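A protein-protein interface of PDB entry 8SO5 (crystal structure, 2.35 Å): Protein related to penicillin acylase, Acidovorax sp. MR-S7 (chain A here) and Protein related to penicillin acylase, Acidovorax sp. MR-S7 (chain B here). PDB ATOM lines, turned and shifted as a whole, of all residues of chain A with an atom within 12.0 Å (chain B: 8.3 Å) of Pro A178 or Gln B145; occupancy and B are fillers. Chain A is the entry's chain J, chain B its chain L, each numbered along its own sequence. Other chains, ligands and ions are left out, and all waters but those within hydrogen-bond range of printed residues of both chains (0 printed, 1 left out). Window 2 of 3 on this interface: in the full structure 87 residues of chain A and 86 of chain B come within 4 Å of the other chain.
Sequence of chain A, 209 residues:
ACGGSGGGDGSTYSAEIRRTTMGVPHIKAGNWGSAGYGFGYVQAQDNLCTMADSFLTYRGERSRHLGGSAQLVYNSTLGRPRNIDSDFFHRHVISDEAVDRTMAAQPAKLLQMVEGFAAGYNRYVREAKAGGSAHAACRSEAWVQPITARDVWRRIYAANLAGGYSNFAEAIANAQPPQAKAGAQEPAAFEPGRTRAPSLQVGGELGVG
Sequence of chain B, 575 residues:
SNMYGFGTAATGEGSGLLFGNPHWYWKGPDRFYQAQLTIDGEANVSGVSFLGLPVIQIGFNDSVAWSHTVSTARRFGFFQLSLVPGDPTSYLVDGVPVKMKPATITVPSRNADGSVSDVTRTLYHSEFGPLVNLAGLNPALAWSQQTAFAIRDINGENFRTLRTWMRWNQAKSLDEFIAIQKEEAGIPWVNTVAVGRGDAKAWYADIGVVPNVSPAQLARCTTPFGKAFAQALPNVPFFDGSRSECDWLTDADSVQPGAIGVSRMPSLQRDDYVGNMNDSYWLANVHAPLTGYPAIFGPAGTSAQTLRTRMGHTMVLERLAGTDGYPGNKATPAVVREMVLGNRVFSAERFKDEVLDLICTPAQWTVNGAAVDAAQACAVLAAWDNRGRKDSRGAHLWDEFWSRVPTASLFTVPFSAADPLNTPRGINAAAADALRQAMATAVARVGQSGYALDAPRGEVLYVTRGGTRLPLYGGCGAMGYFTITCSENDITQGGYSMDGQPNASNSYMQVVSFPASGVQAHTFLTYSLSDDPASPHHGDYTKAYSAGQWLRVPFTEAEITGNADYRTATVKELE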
ATOM      1  N   ASN A 174     -11.017  39.938  27.620  1.00  0.00           N
ATOM      2  CA  ASN A 174     -10.117  39.311  28.574  1.00  0.00           C
ATOM      3  C   ASN A 174     -10.171  37.789  28.444  1.00  0.00           C
ATOM      4  O   ASN A 174      -9.732  37.074  29.342  1.00  0.00           O
ATOM      5  CB  ASN A 174     -10.431  39.741  30.010  1.00  0.00           C
ATOM      6  CG  ASN A 174      -9.959  41.145  30.320  1.00  0.00           C
ATOM      7  OD1 ASN A 174      -8.759  41.409  30.347  1.00  0.00           O
ATOM      8  ND2 ASN A 174     -10.891  42.052  30.561  1.00  0.00           N
ATOM      9  N   ALA A 175     -10.703  37.301  27.319  1.00  0.00           N
ATOM     10  CA  ALA A 175     -10.733  35.873  27.053  1.00  0.00           C
ATOM     11  C   ALA A 175      -9.348  35.414  26.606  1.00  0.00           C
ATOM     12  O   ALA A 175      -8.959  35.619  25.458  1.00  0.00           O
ATOM     13  CB  ALA A 175     -11.788  35.559  26.020  1.00  0.00           C
ATOM     14  N   GLN A 176      -8.611  34.791  27.531  1.00  0.00           N
ATOM     15  CA  GLN A 176      -7.231  34.402  27.291  1.00  0.00           C
ATOM     16  C   GLN A 176      -7.041  32.932  27.659  1.00  0.00           C
ATOM     17  O   GLN A 176      -7.609  32.454  28.639  1.00  0.00           O
ATOM     18  CB  GLN A 176      -6.289  35.288  28.110  1.00  0.00           C
ATOM     19  CG  GLN A 176      -6.132  36.701  27.565  1.00  0.00           C
ATOM     20  CD  GLN A 176      -5.021  36.805  26.549  1.00  0.00           C
ATOM     21  OE1 GLN A 176      -3.999  37.444  26.786  1.00  0.00           O
ATOM     22  NE2 GLN A 176      -5.209  36.165  25.406  1.00  0.00           N
ATOM     23  N   PRO A 177      -6.234  32.171  26.886  1.00  0.00           N
ATOM     24  CA  PRO A 177      -5.936  30.778  27.221  1.00  0.00           C
ATOM     25  C   PRO A 177      -4.987  30.661  28.411  1.00  0.00           C
ATOM     26  O   PRO A 177      -4.311  31.622  28.768  1.00  0.00           O
ATOM     27  CB  PRO A 177      -5.283  30.238  25.940  1.00  0.00           C
ATOM     28  CG  PRO A 177      -4.650  31.459  25.301  1.00  0.00           C
ATOM     29  CD  PRO A 177      -5.580  32.607  25.642  1.00  0.00           C
ATOM     30  N   PRO A 178      -4.913  29.478  29.062  1.00  0.00           N
ATOM     31  CA  PRO A 178      -4.013  29.273  30.198  1.00  0.00           C
ATOM     32  C   PRO A 178      -2.548  29.499  29.831  1.00  0.00           C
ATOM     33  O   PRO A 178      -2.107  29.112  28.750  1.00  0.00           O
ATOM     34  CB  PRO A 178      -4.247  27.810  30.606  1.00  0.00           C
ATOM     35  CG  PRO A 178      -4.892  27.168  29.391  1.00  0.00           C
ATOM     36  CD  PRO A 178      -5.692  28.275  28.737  1.00  0.00           C
ATOM     37  N   GLN A 179      -1.807  30.131  30.749  1.00  0.00           N
ATOM     38  CA  GLN A 179      -0.396  30.422  30.553  1.00  0.00           C
ATOM     39  C   GLN A 179       0.438  29.175  30.873  1.00  0.00           C
ATOM     40  O   GLN A 179       0.005  28.077  30.473  1.00  0.00           O
ATOM     41  CB  GLN A 179       0.039  31.592  31.441  1.00  0.00           C
ATOM     42  CG  GLN A 179      -0.307  32.962  30.875  1.00  0.00           C
ATOM     43  CD  GLN A 179      -1.777  33.115  30.565  1.00  0.00           C
ATOM     44  OE1 GLN A 179      -2.634  32.967  31.435  1.00  0.00           O
ATOM     45  NE2 GLN A 179      -2.078  33.418  29.313  1.00  0.00           N
ATOM     46  N   LEU B  81     -16.546  24.702  24.432  1.00  0.00           N
ATOM     47  CA  LEU B  81     -15.590  24.105  23.516  1.00  0.00           C
ATOM     48  C   LEU B  81     -14.809  23.002  24.227  1.00  0.00           C
ATOM     49  O   LEU B  81     -14.391  23.168  25.371  1.00  0.00           O
ATOM     50  CB  LEU B  81     -14.646  25.198  23.004  1.00  0.00           C
ATOM     51  CG  LEU B  81     -15.312  26.372  22.289  1.00  0.00           C
ATOM     52  CD1 LEU B  81     -14.272  27.356  21.780  1.00  0.00           C
ATOM     53  CD2 LEU B  81     -16.191  25.889  21.144  1.00  0.00           C
ATOM     54  N   SER B  82     -14.623  21.877  23.529  1.00  0.00           N
ATOM     55  CA  SER B  82     -13.733  20.820  23.983  1.00  0.00           C
ATOM     56  C   SER B  82     -12.372  21.003  23.317  1.00  0.00           C
ATOM     57  O   SER B  82     -12.250  20.869  22.101  1.00  0.00           O
ATOM     58  CB  SER B  82     -14.306  19.457  23.694  1.00  0.00           C
ATOM     59  OG  SER B  82     -15.536  19.265  24.379  1.00  0.00           O
ATOM     60  N   LEU B  83     -11.359  21.313  24.130  1.00  0.00           N
ATOM     61  CA  LEU B  83     -10.067  21.736  23.616  1.00  0.00           C
ATOM     62  C   LEU B  83      -9.223  20.517  23.252  1.00  0.00           C
ATOM     63  O   LEU B  83      -9.382  19.443  23.828  1.00  0.00           O
ATOM     64  CB  LEU B  83      -9.372  22.599  24.672  1.00  0.00           C
ATOM     65  CG  LEU B  83     -10.114  23.877  25.061  1.00  0.00           C
ATOM     66  CD1 LEU B  83      -9.219  24.799  25.873  1.00  0.00           C
ATOM     67  CD2 LEU B  83     -10.642  24.595  23.827  1.00  0.00           C
ATOM     68  N   VAL B  84      -8.328  20.708  22.277  1.00  0.00           N
ATOM     69  CA  VAL B  84      -7.386  19.677  21.879  1.00  0.00           C
ATOM     70  C   VAL B  84      -6.305  19.575  22.949  1.00  0.00           C
ATOM     71  O   VAL B  84      -5.707  20.579  23.331  1.00  0.00           O
ATOM     72  CB  VAL B  84      -6.771  19.980  20.498  1.00  0.00           C
ATOM     73  CG1 VAL B  84      -5.657  19.002  20.150  1.00  0.00           C
ATOM     74  CG2 VAL B  84      -7.825  20.008  19.403  1.00  0.00           C
ATOM     75  N   PRO B  85      -6.026  18.361  23.474  1.00  0.00           N
ATOM     76  CA  PRO B  85      -4.939  18.172  24.433  1.00  0.00           C
ATOM     77  C   PRO B  85      -3.603  18.645  23.862  1.00  0.00           C
ATOM     78  O   PRO B  85      -3.129  18.115  22.860  1.00  0.00           O
ATOM     79  CB  PRO B  85      -4.924  16.657  24.697  1.00  0.00           C
ATOM     80  CG  PRO B  85      -5.727  16.053  23.557  1.00  0.00           C
ATOM     81  CD  PRO B  85      -6.739  17.112  23.175  1.00  0.00           C
ATOM     82  N   GLY B  86      -3.017  19.659  24.510  1.00  0.00           N
ATOM     83  CA  GLY B  86      -1.737  20.206  24.094  1.00  0.00           C
ATOM     84  C   GLY B  86      -1.869  21.615  23.521  1.00  0.00           C
ATOM     85  O   GLY B  86      -0.905  22.376  23.523  1.00  0.00           O
ATOM     86  N   ASP B  87      -3.069  21.946  23.030  1.00  0.00           N
ATOM     87  CA  ASP B  87      -3.313  23.225  22.385  1.00  0.00           C
ATOM     88  C   ASP B  87      -4.623  23.816  22.898  1.00  0.00           C
ATOM     89  O   ASP B  87      -5.696  23.486  22.398  1.00  0.00           O
ATOM     90  CB  ASP B  87      -3.343  23.074  20.861  1.00  0.00           C
ATOM     91  CG  ASP B  87      -3.399  24.397  20.118  1.00  0.00           C
ATOM     92  OD1 ASP B  87      -3.366  25.447  20.790  1.00  0.00           O
ATOM     93  OD2 ASP B  87      -3.473  24.365  18.875  1.00  0.00           O
ATOM     94  N   PRO B  88      -4.574  24.701  23.917  1.00  0.00           N
ATOM     95  CA  PRO B  88      -5.774  25.368  24.425  1.00  0.00           C
ATOM     96  C   PRO B  88      -6.404  26.341  23.430  1.00  0.00           C
ATOM     97  O   PRO B  88      -7.436  26.941  23.722  1.00  0.00           O
ATOM     98  CB  PRO B  88      -5.279  26.141  25.660  1.00  0.00           C
ATOM     99  CG  PRO B  88      -3.937  25.517  25.998  1.00  0.00           C
ATOM    100  CD  PRO B  88      -3.367  25.071  24.668  1.00  0.00           C
ATOM    101  N   THR B  89      -5.773  26.494  22.259  1.00  0.00           N
ATOM    102  CA  THR B  89      -6.247  27.429  21.250  1.00  0.00           C
ATOM    103  C   THR B  89      -6.793  26.666  20.045  1.00  0.00           C
ATOM    104  O   THR B  89      -6.988  27.243  18.977  1.00  0.00           O
ATOM    105  CB  THR B  89      -5.144  28.412  20.834  1.00  0.00           C
ATOM    106  OG1 THR B  89      -4.029  27.665  20.344  1.00  0.00           O
ATOM    107  CG2 THR B  89      -4.701  29.307  21.970  1.00  0.00           C
ATOM    108  N   SER B  90      -7.029  25.364  20.232  1.00  0.00           N
ATOM    109  CA  SER B  90      -7.720  24.549  19.246  1.00  0.00           C
ATOM    110  C   SER B  90      -8.863  23.803  19.926  1.00  0.00           C
ATOM    111  O   SER B  90      -8.732  23.375  21.070  1.00  0.00           O
ATOM    112  CB  SER B  90      -6.776  23.593  18.560  1.00  0.00           C
ATOM    113  OG  SER B  90      -5.830  24.291  17.764  1.00  0.00           O
ATOM    114  N   TYR B 124      -9.022  35.657  20.474  1.00  0.00           N
ATOM    115  CA  TYR B 124      -9.334  34.587  19.540  1.00  0.00           C
ATOM    116  C   TYR B 124     -10.814  34.591  19.175  1.00  0.00           C
ATOM    117  O   TYR B 124     -11.652  35.049  19.948  1.00  0.00           O
ATOM    118  CB  TYR B 124      -8.951  33.231  20.137  1.00  0.00           C
ATOM    119  CG  TYR B 124      -7.499  33.105  20.522  1.00  0.00           C
ATOM    120  CD1 TYR B 124      -7.000  33.739  21.646  1.00  0.00           C
ATOM    121  CD2 TYR B 124      -6.618  32.367  19.750  1.00  0.00           C
ATOM    122  CE1 TYR B 124      -5.666  33.632  22.003  1.00  0.00           C
ATOM    123  CE2 TYR B 124      -5.280  32.250  20.090  1.00  0.00           C
ATOM    124  CZ  TYR B 124      -4.803  32.885  21.222  1.00  0.00           C
ATOM    125  OH  TYR B 124      -3.479  32.776  21.567  1.00  0.00           O
ATOM    126  N   ALA B 142     -13.437  28.753  33.949  1.00  0.00           N
ATOM    127  CA  ALA B 142     -12.177  29.313  33.493  1.00  0.00           C
ATOM    128  C   ALA B 142     -11.708  28.590  32.233  1.00  0.00           C
ATOM    129  O   ALA B 142     -11.906  27.386  32.088  1.00  0.00           O
ATOM    130  CB  ALA B 142     -11.148  29.226  34.593  1.00  0.00           C
ATOM    131  N   TRP B 143     -11.087  29.352  31.327  1.00  0.00           N
ATOM    132  CA  TRP B 143     -10.469  28.802  30.133  1.00  0.00           C
ATOM    133  C   TRP B 143      -9.271  27.949  30.547  1.00  0.00           C
ATOM    134  O   TRP B 143      -8.261  28.476  31.009  1.00  0.00           O
ATOM    135  CB  TRP B 143     -10.078  29.943  29.185  1.00  0.00           C
ATOM    136  CG  TRP B 143      -9.525  29.518  27.858  1.00  0.00           C
ATOM    137  CD1 TRP B 143      -9.048  28.288  27.507  1.00  0.00           C
ATOM    138  CD2 TRP B 143      -9.407  30.342  26.684  1.00  0.00           C
ATOM    139  NE1 TRP B 143      -8.633  28.294  26.201  1.00  0.00           N
ATOM    140  CE2 TRP B 143      -8.841  29.539  25.671  1.00  0.00           C
ATOM    141  CE3 TRP B 143      -9.719  31.674  26.394  1.00  0.00           C
ATOM    142  CZ2 TRP B 143      -8.586  30.030  24.391  1.00  0.00           C
ATOM    143  CZ3 TRP B 143      -9.464  32.158  25.130  1.00  0.00           C
ATOM    144  CH2 TRP B 143      -8.905  31.346  24.145  1.00  0.00           C
ATOM    145  N   SER B 144      -9.407  26.628  30.387  1.00  0.00           N
ATOM    146  CA  SER B 144      -8.429  25.683  30.900  1.00  0.00           C
ATOM    147  C   SER B 144      -7.806  24.888  29.755  1.00  0.00           C
ATOM    148  O   SER B 144      -7.828  25.320  28.606  1.00  0.00           O
ATOM    149  CB  SER B 144      -9.059  24.765  31.917  1.00  0.00           C
ATOM    150  OG  SER B 144     -10.098  23.995  31.330  1.00  0.00           O
ATOM    151  N   GLN B 145      -7.250  23.720  30.095  1.00  0.00           N
ATOM    152  CA  GLN B 145      -6.654  22.830  29.113  1.00  0.00           C
ATOM    153  C   GLN B 145      -7.756  21.997  28.462  1.00  0.00           C
ATOM    154  O   GLN B 145      -7.605  21.537  27.333  1.00  0.00           O
ATOM    155  CB  GLN B 145      -5.625  21.910  29.776  1.00  0.00           C
ATOM    156  CG  GLN B 145      -4.677  22.621  30.732  1.00  0.00           C
ATOM    157  CD  GLN B 145      -3.566  23.365  30.032  1.00  0.00           C
ATOM    158  OE1 GLN B 145      -2.796  24.093  30.653  1.00  0.00           O
ATOM    159  NE2 GLN B 145      -3.470  23.184  28.723  1.00  0.00           N
ATOM    160  N   GLN B 146      -8.862  21.816  29.193  1.00  0.00           N
ATOM    161  CA  GLN B 146      -9.924  20.917  28.773  1.00  0.00           C
ATOM    162  C   GLN B 146     -10.995  21.676  27.994  1.00  0.00           C
ATOM    163  O   GLN B 146     -11.412  21.232  26.927  1.00  0.00           O
ATOM    164  CB  GLN B 146     -10.563  20.221  29.977  1.00  0.00           C
ATOM    165  CG  GLN B 146      -9.692  19.143  30.608  1.00  0.00           C
ATOM    166  CD  GLN B 146      -8.645  19.710  31.536  1.00  0.00           C
ATOM    167  OE1 GLN B 146      -8.952  20.430  32.484  1.00  0.00           O
ATOM    168  NE2 GLN B 146      -7.391  19.383  31.269  1.00  0.00           N
ATOM    169  N   THR B 147     -11.451  22.810  28.542  1.00  0.00           N
ATOM    170  CA  THR B 147     -12.640  23.463  28.022  1.00  0.00           C
ATOM    171  C   THR B 147     -12.446  24.974  27.945  1.00  0.00           C
ATOM    172  O   THR B 147     -11.736  25.566  28.757  1.00  0.00           O
ATOM    173  CB  THR B 147     -13.866  23.138  28.884  1.00  0.00           C
ATOM    174  OG1 THR B 147     -13.819  23.962  30.049  1.00  0.00           O
ATOM    175  CG2 THR B 147     -13.937  21.681  29.286  1.00  0.00           C
ATOM    176  N   ALA B 148     -13.100  25.579  26.948  1.00  0.00           N
ATOM    177  CA  ALA B 148     -13.213  27.022  26.830  1.00  0.00           C
ATOM    178  C   ALA B 148     -14.637  27.363  26.403  1.00  0.00           C
ATOM    179  O   ALA B 148     -15.438  26.467  26.148  1.00  0.00           O
ATOM    180  CB  ALA B 148     -12.195  27.547  25.848  1.00  0.00           C
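O of Pro A177 is in hydrogen-bond range of NE2 of Gln A179 (2.9 Å). OD1 of Asp B87 lies close to N of Thr B89 (3.0 Å). The indole nitrogen of Trp B143 lies within hydrogen-bond range of the backbone carbonyl oxygen of Pro B88 (3.1 Å). The backbone NH (N) of Gln B146 is in hydrogen-bond range of the side-chain hydroxyl (OG) of Ser B144, at 3.3 Å. The side-chain hydroxyl (OG) of Ser B144 is in hydrogen-bond range of the backbone NH (N) of Thr B147 (3.3 Å).
Of chain B, only Pro B88 (3.8 Å), Trp B143 (3.4 Å), Ser B144 (3.6 Å) and Gln B145 (3.9 Å) come within 4 Å of Pro A178. Of the printed residues of chain A, Gln B145 touches Pro A178. No residue of chain A comes within 4 Å of Leu B83. No residue of chain A comes within 4 Å of Pro B85. No residue of chain A comes within 4 Å of Gly B86. Of chain A, only Ala A175 (3.5 Å), Gln A176 (3.2 Å), Pro A177 (3.5 Å) and Pro A178 (3.4 Å) come within 4 Å of Trp B143. Of chain A, only Pro A178 (3.6 Å) comes within 4 Å of Ser B144. No residue of chain A comes within 4 Å of Gln B146. No residue of chain A comes within 4 Å of Thr B147. Printed residues of chain B within 4 Å of Pro A177: Thr B89 (3.97 Å), Tyr B124 (3.8 Å) and Trp B143 (3.5 Å). Of the printed residues of chain B, Gln A176 touches Trp B143 (3.2 Å). Of the printed residues of chain A, Thr B89 touches Pro A177 (3.97 Å). Of the printed residues of chain A, Tyr B124 touches Pro A177. Printed residues of chain B within 4 Å of Ala A175: Trp B143. Ser B90 touches none of the printed residues of chain A. The nearest residue of chain B that does not touch Pro A178 is Leu B83 (5.7 Å). The nearest residue of chain A that does not touch Gln B145 is Gln A179 (4.9 Å). The nearest printed residue of chain B that does not touch Gln A176 is Tyr B124 (4.3 Å).
Ala A175 touches Trp B143 (O to CZ3, 3.5 Å). Trp B143 touches Gln A176 (CE3 to O, 3.2 Å). Pro A177 touches Thr B89. Pro A177 touches Tyr B124 (CD to CE1, 3.8 Å). CE2 of Trp B143 touches CA of Pro A177, at 3.5 Å. Pro A178 touches Pro B88. CD of Pro A178 touches O of Trp B143 (3.4 Å). O of Ser B144 touches CG of Pro A178, 3.6 Å away. CG of Pro A178 touches OE1 of Gln B145 (3.9 Å).
Printed residues of chain A that touch a printed residue of chain B: Ala A175, Gln A176, Pro A177 and Pro A178. Hydrophobic or aromatic side chains of chain B within 4 Å of the printed part of chain A: Pro B88, Tyr B124 and Trp B143. Among the printed residues, 9 pairs touch across the chains. Among the printed residues, no Asp or Glu carboxylate lies within 4 Å of a Lys or Arg side-chain nitrogen of the other chain.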
